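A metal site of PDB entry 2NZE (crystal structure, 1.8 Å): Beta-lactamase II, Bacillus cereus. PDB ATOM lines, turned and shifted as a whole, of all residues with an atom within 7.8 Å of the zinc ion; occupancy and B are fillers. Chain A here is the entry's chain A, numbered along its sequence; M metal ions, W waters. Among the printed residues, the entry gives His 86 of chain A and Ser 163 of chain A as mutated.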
ATOM      1  N   HIS A  81      13.028   8.802  23.316  1.00  0.00           N
ATOM      2  CA  HIS A  81      13.827   8.054  22.349  1.00  0.00           C
ATOM      3  C   HIS A  81      13.145   8.054  20.971  1.00  0.00           C
ATOM      4  O   HIS A  81      12.039   8.573  20.830  1.00  0.00           O
ATOM      5  CB  HIS A  81      14.245   6.660  22.861  1.00  0.00           C
ATOM      6  CG  HIS A  81      13.132   5.645  22.885  1.00  0.00           C
ATOM      7  ND1 HIS A  81      12.235   5.549  23.922  1.00  0.00           N
ATOM      8  CD2 HIS A  81      12.829   4.652  22.016  1.00  0.00           C
ATOM      9  CE1 HIS A  81      11.399   4.554  23.670  1.00  0.00           C
ATOM     10  NE2 HIS A  81      11.741   4.006  22.523  1.00  0.00           N
ATOM     11  N   ALA A  82      13.823   7.503  19.970  1.00  0.00           N
ATOM     12  CA  ALA A  82      13.436   7.721  18.588  1.00  0.00           C
ATOM     13  C   ALA A  82      12.530   6.665  17.977  1.00  0.00           C
ATOM     14  O   ALA A  82      12.156   6.790  16.789  1.00  0.00           O
ATOM     15  CB  ALA A  82      14.675   7.905  17.733  1.00  0.00           C
ATOM     16  N   HIS A  83      12.114   5.667  18.755  1.00  0.00           N
ATOM     17  CA  HIS A  83      11.203   4.664  18.213  1.00  0.00           C
ATOM     18  C   HIS A  83       9.958   5.313  17.708  1.00  0.00           C
ATOM     19  O   HIS A  83       9.521   6.333  18.253  1.00  0.00           O
ATOM     20  CB  HIS A  83      10.829   3.573  19.246  1.00  0.00           C
ATOM     21  CG  HIS A  83      11.801   2.438  19.294  1.00  0.00           C
ATOM     22  ND1 HIS A  83      11.957   1.632  20.416  1.00  0.00           N
ATOM     23  CD2 HIS A  83      12.653   1.947  18.365  1.00  0.00           C
ATOM     24  CE1 HIS A  83      12.867   0.709  20.168  1.00  0.00           C
ATOM     25  NE2 HIS A  83      13.316   0.884  18.934  1.00  0.00           N
ATOM     26  N   ALA A  84       9.367   4.711  16.678  1.00  0.00           N
ATOM     27  CA  ALA A  84       8.066   5.142  16.115  1.00  0.00           C
ATOM     28  C   ALA A  84       7.046   5.544  17.173  1.00  0.00           C
ATOM     29  O   ALA A  84       6.296   6.508  16.986  1.00  0.00           O
ATOM     30  CB  ALA A  84       7.470   4.047  15.208  1.00  0.00           C
ATOM     31  N   ASP A  85       6.981   4.800  18.275  1.00  0.00           N
ATOM     32  CA  ASP A  85       5.952   5.101  19.279  1.00  0.00           C
ATOM     33  C   ASP A  85       6.284   6.282  20.177  1.00  0.00           C
ATOM     34  O   ASP A  85       5.489   6.651  21.066  1.00  0.00           O
ATOM     35  CB  ASP A  85       5.584   3.868  20.112  1.00  0.00           C
ATOM     36  CG  ASP A  85       6.748   3.303  20.914  1.00  0.00           C
ATOM     37  OD1 ASP A  85       7.890   3.833  20.869  1.00  0.00           O
ATOM     38  OD2 ASP A  85       6.505   2.290  21.600  1.00  0.00           O
ATOM     39  N   HIS A  86       7.475   6.848  19.978  1.00  0.00           N
ATOM     40  CA  HIS A  86       7.887   8.043  20.682  1.00  0.00           C
ATOM     41  C   HIS A  86       8.024   9.252  19.757  1.00  0.00           C
ATOM     42  O   HIS A  86       7.719  10.365  20.148  1.00  0.00           O
ATOM     43  CB  HIS A  86       9.178   7.797  21.454  1.00  0.00           C
ATOM     44  CG  HIS A  86       8.953   6.999  22.692  1.00  0.00           C
ATOM     45  ND1 HIS A  86       9.067   7.552  23.955  1.00  0.00           N
ATOM     46  CD2 HIS A  86       8.508   5.735  22.861  1.00  0.00           C
ATOM     47  CE1 HIS A  86       8.745   6.637  24.851  1.00  0.00           C
ATOM     48  NE2 HIS A  86       8.381   5.532  24.213  1.00  0.00           N
ATOM     49  N   HIS A 144      17.123   0.392  26.697  1.00  0.00           N
ATOM     50  CA  HIS A 144      16.016   0.097  25.823  1.00  0.00           C
ATOM     51  C   HIS A 144      16.373   0.376  24.352  1.00  0.00           C
ATOM     52  O   HIS A 144      16.044  -0.407  23.451  1.00  0.00           O
ATOM     53  CB  HIS A 144      14.798   0.885  26.225  1.00  0.00           C
ATOM     54  CG  HIS A 144      13.699   0.782  25.238  1.00  0.00           C
ATOM     55  ND1 HIS A 144      13.014  -0.406  25.022  1.00  0.00           N
ATOM     56  CD2 HIS A 144      13.194   1.683  24.369  1.00  0.00           C
ATOM     57  CE1 HIS A 144      12.118  -0.221  24.076  1.00  0.00           C
ATOM     58  NE2 HIS A 144      12.206   1.039  23.663  1.00  0.00           N
ATOM     59  N   THR A 145      16.992   1.530  24.123  1.00  0.00           N
ATOM     60  CA  THR A 145      17.598   1.831  22.852  1.00  0.00           C
ATOM     61  C   THR A 145      18.914   2.503  23.102  1.00  0.00           C
ATOM     62  O   THR A 145      19.308   2.786  24.245  1.00  0.00           O
ATOM     63  CB  THR A 145      16.727   2.799  22.055  1.00  0.00           C
ATOM     64  OG1 THR A 145      16.444   3.920  22.887  1.00  0.00           O
ATOM     65  CG2 THR A 145      15.420   2.140  21.607  1.00  0.00           C
ATOM     66  N   ASP A 147      19.539   5.475  22.434  1.00  0.00           N
ATOM     67  CA  ASP A 147      19.418   6.922  22.621  1.00  0.00           C
ATOM     68  C   ASP A 147      18.602   7.334  23.813  1.00  0.00           C
ATOM     69  O   ASP A 147      18.491   8.517  24.105  1.00  0.00           O
ATOM     70  CB  ASP A 147      18.844   7.594  21.368  1.00  0.00           C
ATOM     71  CG  ASP A 147      17.464   7.064  20.985  1.00  0.00           C
ATOM     72  OD1 ASP A 147      17.224   5.829  21.022  1.00  0.00           O
ATOM     73  OD2 ASP A 147      16.618   7.891  20.635  1.00  0.00           O
ATOM     74  N   ASN A 148      18.018   6.357  24.495  1.00  0.00           N
ATOM     75  CA  ASN A 148      17.035   6.631  25.521  1.00  0.00           C
ATOM     76  C   ASN A 148      17.506   7.603  26.590  1.00  0.00           C
ATOM     77  O   ASN A 148      18.623   7.506  27.080  1.00  0.00           O
ATOM     78  CB  ASN A 148      16.437   5.333  26.132  1.00  0.00           C
ATOM     79  CG  ASN A 148      17.498   4.295  26.603  1.00  0.00           C
ATOM     80  OD1 ASN A 148      17.176   3.115  26.654  1.00  0.00           O
ATOM     81  ND2 ASN A 148      18.723   4.718  26.965  1.00  0.00           N
ATOM     82  N   SER A 163      10.911   4.141  28.483  1.00  0.00           N
ATOM     83  CA  SER A 163      11.042   2.731  28.158  1.00  0.00           C
ATOM     84  C   SER A 163      12.216   2.046  28.838  1.00  0.00           C
ATOM     85  O   SER A 163      12.318   0.824  28.806  1.00  0.00           O
ATOM     86  CB  SER A 163      11.093   2.561  26.639  1.00  0.00           C
ATOM     87  OG  SER A 163       9.948   3.138  26.052  1.00  0.00           O
ATOM     88  N   LEU A 164      13.064   2.825  29.508  1.00  0.00           N
ATOM     89  CA  LEU A 164      14.176   2.306  30.325  1.00  0.00           C
ATOM     90  C   LEU A 164      13.688   1.598  31.584  1.00  0.00           C
ATOM     91  O   LEU A 164      14.401   0.807  32.175  1.00  0.00           O
ATOM     92  CB  LEU A 164      15.121   3.444  30.739  1.00  0.00           C
ATOM     93  CG  LEU A 164      16.560   3.127  31.155  1.00  0.00           C
ATOM     94  CD1 LEU A 164      17.443   2.689  29.947  1.00  0.00           C
ATOM     95  CD2 LEU A 164      17.181   4.348  31.865  1.00  0.00           C
ATOM     96  N   LYS A 166      10.600  -0.518  33.483  1.00  0.00           N
ATOM     97  CA  LYS A 166       9.373  -1.311  33.422  1.00  0.00           C
ATOM     98  C   LYS A 166       8.547  -1.159  34.682  1.00  0.00           C
ATOM     99  O   LYS A 166       9.096  -0.884  35.759  1.00  0.00           O
ATOM    100  CB  LYS A 166       9.711  -2.793  33.178  1.00  0.00           C
ATOM    101  CG  LYS A 166      10.693  -2.992  32.001  1.00  0.00           C
ATOM    102  CD  LYS A 166      10.086  -2.505  30.684  1.00  0.00           C
ATOM    103  CE  LYS A 166      11.182  -1.932  29.814  1.00  0.00           C
ATOM    104  NZ  LYS A 166      10.628  -1.491  28.481  1.00  0.00           N
ATOM    105  N   ASN A 175      10.417  -4.610  23.430  1.00  0.00           N
ATOM    106  CA  ASN A 175      11.198  -4.712  22.209  1.00  0.00           C
ATOM    107  C   ASN A 175      12.682  -4.570  22.518  1.00  0.00           C
ATOM    108  O   ASN A 175      13.119  -3.514  22.968  1.00  0.00           O
ATOM    109  CB  ASN A 175      10.731  -3.634  21.216  1.00  0.00           C
ATOM    110  CG  ASN A 175      11.528  -3.632  19.920  1.00  0.00           C
ATOM    111  OD1 ASN A 175      12.569  -4.254  19.798  1.00  0.00           O
ATOM    112  ND2 ASN A 175      11.045  -2.860  18.944  1.00  0.00           N
ATOM    113  N   ASP A 178      16.326  -3.425  19.388  1.00  0.00           N
ATOM    114  CA  ASP A 178      17.123  -2.209  19.295  1.00  0.00           C
ATOM    115  C   ASP A 178      17.779  -1.913  20.653  1.00  0.00           C
ATOM    116  O   ASP A 178      18.339  -0.828  20.852  1.00  0.00           O
ATOM    117  CB  ASP A 178      16.235  -1.042  18.907  1.00  0.00           C
ATOM    118  CG  ASP A 178      15.711  -1.166  17.483  1.00  0.00           C
ATOM    119  OD1 ASP A 178      16.364  -1.833  16.651  1.00  0.00           O
ATOM    120  OD2 ASP A 178      14.650  -0.598  17.212  1.00  0.00           O
ATOM    121  N   HIS A 205       5.388   2.319  30.490  1.00  0.00           N
ATOM    122  CA  HIS A 205       3.974   1.985  30.588  1.00  0.00           C
ATOM    123  C   HIS A 205       3.705   1.394  31.954  1.00  0.00           C
ATOM    124  O   HIS A 205       4.599   0.787  32.562  1.00  0.00           O
ATOM    125  CB  HIS A 205       3.391   1.065  29.514  1.00  0.00           C
ATOM    126  CG  HIS A 205       4.096   1.070  28.177  1.00  0.00           C
ATOM    127  ND1 HIS A 205       4.231   2.211  27.415  1.00  0.00           N
ATOM    128  CD2 HIS A 205       4.600   0.060  27.438  1.00  0.00           C
ATOM    129  CE1 HIS A 205       4.838   1.897  26.273  1.00  0.00           C
ATOM    130  NE2 HIS A 205       5.071   0.606  26.267  1.00  0.00           N
HETATM  131 ZN    ZN M   1      11.166   2.006  22.203  1.00  0.00          ZN
HETATM  132  O   HOH W   1      10.149  -0.225  21.637  1.00  0.00           O
HETATM  133  O   HOH W   2       9.471   2.264  22.682  1.00  0.00           O
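Residues that only touch the zinc ion: Asp 85 (3.98 Å). The nearest printed residue that does not touch the zinc ion is Ser 163 (4.2 Å).
The zinc ion is bound by water W2 (1.8 Å), ND1 of His 83 (2.0 Å), NE2 of His 144 (2.0 Å), NE2 of His 81 (2.1 Å) and water W1 (2.5 Å). The zinc ion has five donor atoms within binding distance.
A ring nitrogen (NE2) of His 83 lies within hydrogen-bond range of the side-chain carboxylate of Asp 178. The backbone NH of His 144 lies within hydrogen-bond range of the side-chain amide oxygen of Asn 148, at 2.7 Å.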
